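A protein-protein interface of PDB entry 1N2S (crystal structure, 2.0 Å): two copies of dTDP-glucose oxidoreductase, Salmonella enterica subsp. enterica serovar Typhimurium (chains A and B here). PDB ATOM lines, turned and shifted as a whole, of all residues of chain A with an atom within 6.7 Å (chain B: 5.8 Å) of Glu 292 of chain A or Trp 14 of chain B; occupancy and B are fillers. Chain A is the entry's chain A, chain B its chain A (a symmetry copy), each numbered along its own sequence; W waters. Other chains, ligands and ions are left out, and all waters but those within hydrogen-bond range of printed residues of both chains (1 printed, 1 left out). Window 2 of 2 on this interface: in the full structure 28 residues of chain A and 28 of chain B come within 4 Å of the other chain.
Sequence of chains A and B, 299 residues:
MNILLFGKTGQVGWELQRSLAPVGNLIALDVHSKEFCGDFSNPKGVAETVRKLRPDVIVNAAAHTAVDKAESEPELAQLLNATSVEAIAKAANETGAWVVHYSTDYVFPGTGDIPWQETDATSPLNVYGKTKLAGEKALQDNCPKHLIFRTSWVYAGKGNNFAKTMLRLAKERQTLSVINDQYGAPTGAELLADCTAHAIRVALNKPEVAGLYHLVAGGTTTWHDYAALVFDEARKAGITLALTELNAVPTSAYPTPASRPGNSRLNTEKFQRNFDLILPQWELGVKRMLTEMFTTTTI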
ATOM      1  N   GLY A 157       3.323  18.748 -13.630  1.00  0.00           N
ATOM      2  CA  GLY A 157       2.110  19.401 -13.132  1.00  0.00           C
ATOM      3  C   GLY A 157       0.845  18.758 -13.666  1.00  0.00           C
ATOM      4  O   GLY A 157      -0.227  18.948 -13.136  1.00  0.00           O
ATOM      5  N   GLU A 190       9.765  19.347 -16.845  1.00  0.00           N
ATOM      6  CA  GLU A 190      10.105  20.514 -17.648  1.00  0.00           C
ATOM      7  C   GLU A 190      11.611  20.581 -17.792  1.00  0.00           C
ATOM      8  O   GLU A 190      12.097  20.644 -18.927  1.00  0.00           O
ATOM      9  CB  GLU A 190       9.622  21.861 -17.016  1.00  0.00           C
ATOM     10  CG  GLU A 190       8.139  22.028 -16.978  1.00  0.00           C
ATOM     11  CD  GLU A 190       7.708  23.332 -16.346  1.00  0.00           C
ATOM     12  OE1 GLU A 190       8.433  23.748 -15.474  1.00  0.00           O
ATOM     13  OE2 GLU A 190       6.650  23.949 -16.692  1.00  0.00           O
ATOM     14  N   LYS A 287       8.037  25.365  -7.261  1.00  0.00           N
ATOM     15  CA  LYS A 287       7.224  26.567  -6.996  1.00  0.00           C
ATOM     16  C   LYS A 287       6.450  26.966  -8.293  1.00  0.00           C
ATOM     17  O   LYS A 287       5.289  27.438  -8.294  1.00  0.00           O
ATOM     18  CB  LYS A 287       8.121  27.721  -6.510  1.00  0.00           C
ATOM     19  CG  LYS A 287       8.680  27.673  -5.045  1.00  0.00           C
ATOM     20  CD  LYS A 287       9.645  28.865  -4.787  1.00  0.00           C
ATOM     21  CE  LYS A 287      10.204  28.876  -3.356  1.00  0.00           C
ATOM     22  NZ  LYS A 287      11.263  29.922  -3.119  1.00  0.00           N
ATOM     23  N   ARG A 288       7.084  26.691  -9.416  1.00  0.00           N
ATOM     24  CA  ARG A 288       6.471  27.039 -10.659  1.00  0.00           C
ATOM     25  C   ARG A 288       5.331  26.091 -10.919  1.00  0.00           C
ATOM     26  O   ARG A 288       4.321  26.544 -11.323  1.00  0.00           O
ATOM     27  CB  ARG A 288       7.465  26.949 -11.796  1.00  0.00           C
ATOM     28  CG  ARG A 288       6.879  26.895 -13.233  1.00  0.00           C
ATOM     29  CD  ARG A 288       7.962  26.678 -14.309  1.00  0.00           C
ATOM     30  NE  ARG A 288       7.319  26.605 -15.608  1.00  0.00           N
ATOM     31  CZ  ARG A 288       6.970  27.639 -16.365  1.00  0.00           C
ATOM     32  NH1 ARG A 288       7.235  28.862 -16.007  1.00  0.00           N
ATOM     33  NH2 ARG A 288       6.361  27.452 -17.530  1.00  0.00           N
ATOM     34  N   MET A 289       5.508  24.779 -10.726  1.00  0.00           N
ATOM     35  CA  MET A 289       4.399  23.910 -10.941  1.00  0.00           C
ATOM     36  C   MET A 289       3.277  24.221  -9.933  1.00  0.00           C
ATOM     37  O   MET A 289       2.112  24.208 -10.317  1.00  0.00           O
ATOM     38  CB  MET A 289       4.826  22.446 -11.080  1.00  0.00           C
ATOM     39  CG  MET A 289       5.141  21.716  -9.988  1.00  0.00           C
ATOM     40  SD  MET A 289       4.000  20.253  -9.834  1.00  0.00           S
ATOM     41  CE  MET A 289       4.510  19.776  -8.136  1.00  0.00           C
ATOM     42  N   LEU A 290       3.635  24.590  -8.703  1.00  0.00           N
ATOM     43  CA  LEU A 290       2.624  24.948  -7.701  1.00  0.00           C
ATOM     44  C   LEU A 290       1.823  26.174  -8.149  1.00  0.00           C
ATOM     45  O   LEU A 290       0.587  26.149  -8.128  1.00  0.00           O
ATOM     46  CB  LEU A 290       3.240  25.121  -6.324  1.00  0.00           C
ATOM     47  CG  LEU A 290       3.788  23.806  -5.744  1.00  0.00           C
ATOM     48  CD1 LEU A 290       4.675  24.091  -4.570  1.00  0.00           C
ATOM     49  CD2 LEU A 290       2.675  22.854  -5.400  1.00  0.00           C
ATOM     50  N   THR A 291       2.506  27.208  -8.621  1.00  0.00           N
ATOM     51  CA  THR A 291       1.798  28.382  -9.115  1.00  0.00           C
ATOM     52  C   THR A 291       0.845  28.054 -10.256  1.00  0.00           C
ATOM     53  O   THR A 291      -0.289  28.547 -10.317  1.00  0.00           O
ATOM     54  CB  THR A 291       2.758  29.403  -9.580  1.00  0.00           C
ATOM     55  OG1 THR A 291       3.518  29.866  -8.450  1.00  0.00           O
ATOM     56  CG2 THR A 291       1.982  30.608  -9.965  1.00  0.00           C
ATOM     57  N   GLU A 292       1.308  27.219 -11.158  1.00  0.00           N
ATOM     58  CA  GLU A 292       0.485  26.862 -12.301  1.00  0.00           C
ATOM     59  C   GLU A 292      -0.728  26.138 -11.803  1.00  0.00           C
ATOM     60  O   GLU A 292      -1.834  26.376 -12.263  1.00  0.00           O
ATOM     61  CB  GLU A 292       1.249  25.991 -13.308  1.00  0.00           C
ATOM     62  CG  GLU A 292       2.119  26.785 -14.243  1.00  0.00           C
ATOM     63  CD  GLU A 292       2.747  25.936 -15.401  1.00  0.00           C
ATOM     64  OE1 GLU A 292       2.837  24.686 -15.280  1.00  0.00           O
ATOM     65  OE2 GLU A 292       3.062  26.501 -16.462  1.00  0.00           O
ATOM     66  N   MET A 293      -0.536  25.243 -10.853  1.00  0.00           N
ATOM     67  CA  MET A 293      -1.686  24.550 -10.289  1.00  0.00           C
ATOM     68  C   MET A 293      -2.601  25.557  -9.564  1.00  0.00           C
ATOM     69  O   MET A 293      -3.807  25.484  -9.700  1.00  0.00           O
ATOM     70  CB  MET A 293      -1.225  23.462  -9.298  1.00  0.00           C
ATOM     71  CG  MET A 293      -0.432  22.309  -9.865  1.00  0.00           C
ATOM     72  SD  MET A 293       0.130  21.187  -8.492  1.00  0.00           S
ATOM     73  CE  MET A 293      -1.377  21.370  -7.385  1.00  0.00           C
ATOM     74  N   PHE A 294      -2.048  26.489  -8.787  1.00  0.00           N
ATOM     75  CA  PHE A 294      -2.873  27.402  -8.022  1.00  0.00           C
ATOM     76  C   PHE A 294      -3.519  28.521  -8.856  1.00  0.00           C
ATOM     77  O   PHE A 294      -4.614  28.875  -8.580  1.00  0.00           O
ATOM     78  CB  PHE A 294      -2.094  27.995  -6.830  1.00  0.00           C
ATOM     79  CG  PHE A 294      -1.562  26.959  -5.872  1.00  0.00           C
ATOM     80  CD1 PHE A 294      -2.149  25.716  -5.766  1.00  0.00           C
ATOM     81  CD2 PHE A 294      -0.474  27.222  -5.122  1.00  0.00           C
ATOM     82  CE1 PHE A 294      -1.656  24.760  -4.916  1.00  0.00           C
ATOM     83  CE2 PHE A 294       0.017  26.279  -4.228  1.00  0.00           C
ATOM     84  CZ  PHE A 294      -0.599  25.054  -4.106  1.00  0.00           C
ATOM     85  N   THR A 295      -2.842  29.056  -9.865  1.00  0.00           N
ATOM     86  CA  THR A 295      -3.394  30.127 -10.687  1.00  0.00           C
ATOM     87  C   THR A 295      -3.900  29.488 -11.971  1.00  0.00           C
ATOM     88  O   THR A 295      -3.405  29.698 -13.057  1.00  0.00           O
ATOM     89  CB  THR A 295      -2.335  31.184 -10.978  1.00  0.00           C
ATOM     90  OG1 THR A 295      -1.236  30.595 -11.725  1.00  0.00           O
ATOM     91  CG2 THR A 295      -1.696  31.660  -9.671  1.00  0.00           C
ATOM     92  N   THR A 296      -4.921  28.672 -11.808  1.00  0.00           N
ATOM     93  CA  THR A 296      -5.482  27.894 -12.905  1.00  0.00           C
ATOM     94  C   THR A 296      -6.627  28.617 -13.589  1.00  0.00           C
ATOM     95  O   THR A 296      -7.773  28.426 -13.198  1.00  0.00           O
ATOM     96  CB  THR A 296      -5.992  26.547 -12.319  1.00  0.00           C
ATOM     97  OG1 THR A 296      -7.250  26.182 -12.904  1.00  0.00           O
ATOM     98  CG2 THR A 296      -6.342  26.692 -10.859  1.00  0.00           C
ATOM     99  N   THR A 297      -6.358  29.465 -14.583  1.00  0.00           N
ATOM    100  CA  THR A 297      -7.487  30.123 -15.248  1.00  0.00           C
ATOM    101  C   THR A 297      -8.401  29.001 -15.679  1.00  0.00           C
ATOM    102  O   THR A 297      -8.023  28.143 -16.478  1.00  0.00           O
ATOM    103  CB  THR A 297      -7.076  31.013 -16.456  1.00  0.00           C
ATOM    104  OG1 THR A 297      -7.249  32.398 -16.117  1.00  0.00           O
ATOM    105  CG2 THR A 297      -8.025  30.861 -17.587  1.00  0.00           C
ATOM    106  N   GLY B   7       9.433  41.014 -18.389  1.00  0.00           N
ATOM    107  CA  GLY B   7       8.103  40.520 -18.774  1.00  0.00           C
ATOM    108  C   GLY B   7       7.823  39.078 -18.400  1.00  0.00           C
ATOM    109  O   GLY B   7       7.037  38.380 -19.055  1.00  0.00           O
ATOM    110  N   LYS B   8       8.394  38.660 -17.280  1.00  0.00           N
ATOM    111  CA  LYS B   8       8.355  37.287 -16.806  1.00  0.00           C
ATOM    112  C   LYS B   8       6.957  36.766 -16.546  1.00  0.00           C
ATOM    113  O   LYS B   8       6.778  35.597 -16.725  1.00  0.00           O
ATOM    114  CB  LYS B   8       9.144  37.098 -15.501  1.00  0.00           C
ATOM    115  CG  LYS B   8       8.552  37.797 -14.326  1.00  0.00           C
ATOM    116  CD  LYS B   8       9.212  37.244 -13.100  1.00  0.00           C
ATOM    117  CE  LYS B   8       8.762  37.823 -11.793  1.00  0.00           C
ATOM    118  NZ  LYS B   8       9.867  37.382 -10.875  1.00  0.00           N
ATOM    119  N   THR B   9       6.005  37.632 -16.175  1.00  0.00           N
ATOM    120  CA  THR B   9       4.644  37.206 -15.929  1.00  0.00           C
ATOM    121  C   THR B   9       3.745  37.134 -17.156  1.00  0.00           C
ATOM    122  O   THR B   9       2.622  36.691 -17.029  1.00  0.00           O
ATOM    123  CB  THR B   9       3.921  38.081 -14.848  1.00  0.00           C
ATOM    124  OG1 THR B   9       3.608  39.379 -15.396  1.00  0.00           O
ATOM    125  CG2 THR B   9       4.832  38.391 -13.686  1.00  0.00           C
ATOM    126  N   GLY B  10       4.203  37.566 -18.327  1.00  0.00           N
ATOM    127  CA  GLY B  10       3.342  37.512 -19.492  1.00  0.00           C
ATOM    128  C   GLY B  10       3.189  36.100 -20.042  1.00  0.00           C
ATOM    129  O   GLY B  10       3.753  35.158 -19.519  1.00  0.00           O
ATOM    130  N   GLN B  11       2.430  35.981 -21.102  1.00  0.00           N
ATOM    131  CA  GLN B  11       2.223  34.681 -21.743  1.00  0.00           C
ATOM    132  C   GLN B  11       3.548  34.144 -22.171  1.00  0.00           C
ATOM    133  O   GLN B  11       3.916  33.033 -21.835  1.00  0.00           O
ATOM    134  CB  GLN B  11       1.403  34.804 -23.016  1.00  0.00           C
ATOM    135  CG  GLN B  11      -0.035  35.240 -22.786  1.00  0.00           C
ATOM    136  CD  GLN B  11      -0.872  35.119 -24.050  1.00  0.00           C
ATOM    137  OE1 GLN B  11      -1.738  34.309 -24.058  1.00  0.00           O
ATOM    138  NE2 GLN B  11      -0.592  35.918 -25.115  1.00  0.00           N
ATOM    139  N   VAL B  12       4.306  34.915 -22.868  1.00  0.00           N
ATOM    140  CA  VAL B  12       5.564  34.362 -23.428  1.00  0.00           C
ATOM    141  C   VAL B  12       6.569  34.319 -22.310  1.00  0.00           C
ATOM    142  O   VAL B  12       7.257  33.339 -22.152  1.00  0.00           O
ATOM    143  CB  VAL B  12       6.080  35.148 -24.526  1.00  0.00           C
ATOM    144  CG1 VAL B  12       7.357  34.587 -25.029  1.00  0.00           C
ATOM    145  CG2 VAL B  12       5.104  35.234 -25.595  1.00  0.00           C
ATOM    146  N   GLY B  13       6.630  35.404 -21.521  1.00  0.00           N
ATOM    147  CA  GLY B  13       7.489  35.393 -20.383  1.00  0.00           C
ATOM    148  C   GLY B  13       7.368  34.233 -19.434  1.00  0.00           C
ATOM    149  O   GLY B  13       8.385  33.794 -18.915  1.00  0.00           O
ATOM    150  N   TRP B  14       6.136  33.822 -19.097  1.00  0.00           N
ATOM    151  CA  TRP B  14       6.005  32.717 -18.159  1.00  0.00           C
ATOM    152  C   TRP B  14       6.662  31.453 -18.751  1.00  0.00           C
ATOM    153  O   TRP B  14       7.334  30.696 -17.976  1.00  0.00           O
ATOM    154  CB  TRP B  14       4.509  32.445 -17.852  1.00  0.00           C
ATOM    155  CG  TRP B  14       4.293  31.255 -16.947  1.00  0.00           C
ATOM    156  CD1 TRP B  14       3.898  29.996 -17.320  1.00  0.00           C
ATOM    157  CD2 TRP B  14       4.545  31.211 -15.546  1.00  0.00           C
ATOM    158  NE1 TRP B  14       3.828  29.203 -16.208  1.00  0.00           N
ATOM    159  CE2 TRP B  14       4.287  29.897 -15.113  1.00  0.00           C
ATOM    160  CE3 TRP B  14       4.988  32.159 -14.601  1.00  0.00           C
ATOM    161  CZ2 TRP B  14       4.345  29.529 -13.771  1.00  0.00           C
ATOM    162  CZ3 TRP B  14       5.097  31.776 -13.240  1.00  0.00           C
ATOM    163  CH2 TRP B  14       4.807  30.455 -12.857  1.00  0.00           C
ATOM    164  N   GLU B  15       6.510  31.223 -20.075  1.00  0.00           N
ATOM    165  CA  GLU B  15       7.154  30.097 -20.756  1.00  0.00           C
ATOM    166  C   GLU B  15       8.704  30.270 -20.892  1.00  0.00           C
ATOM    167  O   GLU B  15       9.462  29.267 -20.782  1.00  0.00           O
ATOM    168  CB  GLU B  15       6.499  29.704 -22.097  1.00  0.00           C
ATOM    169  CG  GLU B  15       5.151  29.150 -21.793  1.00  0.00           C
ATOM    170  CD  GLU B  15       5.120  27.855 -21.020  1.00  0.00           C
ATOM    171  OE1 GLU B  15       4.331  27.808 -20.049  1.00  0.00           O
ATOM    172  OE2 GLU B  15       5.780  26.869 -21.440  1.00  0.00           O
ATOM    173  N   LEU B  16       9.140  31.530 -20.983  1.00  0.00           N
ATOM    174  CA  LEU B  16      10.581  31.789 -20.969  1.00  0.00           C
ATOM    175  C   LEU B  16      11.225  31.530 -19.649  1.00  0.00           C
ATOM    176  O   LEU B  16      12.396  31.155 -19.582  1.00  0.00           O
ATOM    177  CB  LEU B  16      10.884  33.206 -21.434  1.00  0.00           C
ATOM    178  CG  LEU B  16      10.663  33.456 -22.866  1.00  0.00           C
ATOM    179  CD1 LEU B  16      10.444  34.968 -23.167  1.00  0.00           C
ATOM    180  CD2 LEU B  16      11.854  32.841 -23.689  1.00  0.00           C
ATOM    181  N   GLN B  17      10.503  31.756 -18.564  1.00  0.00           N
ATOM    182  CA  GLN B  17      11.027  31.417 -17.283  1.00  0.00           C
ATOM    183  C   GLN B  17      11.445  29.973 -17.281  1.00  0.00           C
ATOM    184  O   GLN B  17      12.376  29.601 -16.541  1.00  0.00           O
ATOM    185  CB  GLN B  17      10.078  31.682 -16.128  1.00  0.00           C
ATOM    186  CG  GLN B  17       9.838  33.240 -15.798  1.00  0.00           C
ATOM    187  CD  GLN B  17       9.083  33.421 -14.534  1.00  0.00           C
ATOM    188  OE1 GLN B  17       7.987  33.943 -14.511  1.00  0.00           O
ATOM    189  NE2 GLN B  17       9.620  32.925 -13.501  1.00  0.00           N
ATOM    190  N   ARG B  18      10.738  29.124 -17.981  1.00  0.00           N
ATOM    191  CA  ARG B  18      11.056  27.701 -17.992  1.00  0.00           C
ATOM    192  C   ARG B  18      12.171  27.444 -19.012  1.00  0.00           C
ATOM    193  O   ARG B  18      13.196  26.848 -18.646  1.00  0.00           O
ATOM    194  CB  ARG B  18       9.842  26.851 -18.365  1.00  0.00           C
ATOM    195  CG  ARG B  18      10.078  25.501 -18.694  1.00  0.00           C
ATOM    196  CD  ARG B  18       8.881  24.755 -19.387  1.00  0.00           C
ATOM    197  NE  ARG B  18       8.320  25.419 -20.591  1.00  0.00           N
ATOM    198  CZ  ARG B  18       8.971  25.614 -21.720  1.00  0.00           C
ATOM    199  NH1 ARG B  18      10.203  25.142 -21.863  1.00  0.00           N
ATOM    200  NH2 ARG B  18       8.351  26.189 -22.729  1.00  0.00           N
ATOM    201  N   LYS B 158      -1.868  29.345 -19.436  1.00  0.00           N
ATOM    202  CA  LYS B 158      -1.950  30.030 -18.187  1.00  0.00           C
ATOM    203  C   LYS B 158      -2.503  31.448 -18.478  1.00  0.00           C
ATOM    204  O   LYS B 158      -1.960  32.237 -19.299  1.00  0.00           O
ATOM    205  CB  LYS B 158      -0.566  30.166 -17.573  1.00  0.00           C
ATOM    206  CG  LYS B 158      -0.577  30.691 -16.151  1.00  0.00           C
ATOM    207  CD  LYS B 158       0.842  30.975 -15.657  1.00  0.00           C
ATOM    208  CE  LYS B 158       0.897  31.852 -14.478  1.00  0.00           C
ATOM    209  NZ  LYS B 158       0.684  31.114 -13.251  1.00  0.00           N
HETATM  210  O   HOH W   1       8.174  30.016 -13.476  1.00  0.00           O
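No position is printed for both chains.
Of the 7 pairs that touch across the chains among the printed residues, none has its exchanged pair printed and touching as well.
Of the 13 printed residues of chain A, 5 touch a printed residue of chain B.
Among the printed residues, 7 pairs touch across the chains.
Among the printed residues, Asp or Glu carboxylates within 4 Å of a Lys or Arg side-chain nitrogen of the other chain: Arg 288 of chain A with Glu 15 of chain B (3.3 Å).
Glu 292 of chain A touches just one residue of chain B: Trp 14.
Printed residues of chain A within 4 Å of Trp 14 of chain B: Arg 288 (2.7 Å) and Glu 292 (2.8 Å).
Printed residues of chain A within 4 Å of Glu 15 of chain B: Arg 288.
Printed residues of chain A within 4 Å of Arg 18 of chain B: Glu 190 (3.6 Å) and Arg 288 (3.6 Å).
Printed residues of chain B within 4 Å of Arg 288 of chain A: Trp 14 (2.7 Å), Glu 15 (3.3 Å) and Arg 18 (3.6 Å).
Of the printed residues of chain B, Thr 295 of chain A touches Lys 158.
Gly 7 of chain B touches none of the printed residues of chain A.
The nearest printed residue of chain B that does not touch Glu 190 of chain A is Glu 15 of chain B (5.6 Å).
Glu 190 of chain A touches Arg 18 of chain B (CD to CD, 3.6 Å).
Arg 288 of chain A touches Arg 18 of chain B.
Thr 291 of chain A touches Lys 158 of chain B (CG2 to NZ, 3.6 Å).
Water W1 bridges NH1 of Arg 288 of chain A (2.9 Å) and NE2 of Gln 17 of chain B (3.2 Å).
The backbone carbonyl oxygen (O) of Trp 14 of chain B sits at hydrogen-bond distance from the guanidinium group (NH1) of Arg 288 of chain A (2.7 Å).
NH2 of Arg 288 of chain A lies within salt-bridge range of OE1 of Glu 15 of chain B, at 3.3 Å.
The indole nitrogen (NE1) of Trp 14 of chain B sits at hydrogen-bond distance from the side-chain carboxylate (OE2) of Glu 292 of chain A.
The side-chain amino group of Lys 158 of chain B lies within hydrogen-bond range of the side-chain hydroxyl of Thr 295 of chain A.
The side-chain carboxylate (OE2) of Glu 190 of chain A lies within salt-bridge range of the guanidinium group (NE) of Arg 288 of chain A, at 2.9 Å.
O of Lys 287 of chain A sits at hydrogen-bond distance from OG1 of Thr 291 of chain A (3.0 Å).
The guanidinium group of Arg 288 of chain A is in salt-bridge range of the side-chain carboxylate of Glu 292 of chain A, 3.6 Å away.
O of Thr 291 of chain A is in hydrogen-bond range of OG1 of Thr 295 of chain A (2.7 Å).
O of Lys 8 of chain B is in hydrogen-bond range of N of Trp 14 of chain B (3.0 Å).
OE2 of Glu 15 of chain B lies within salt-bridge range of NH2 of Arg 18 of chain B, 3.0 Å away.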
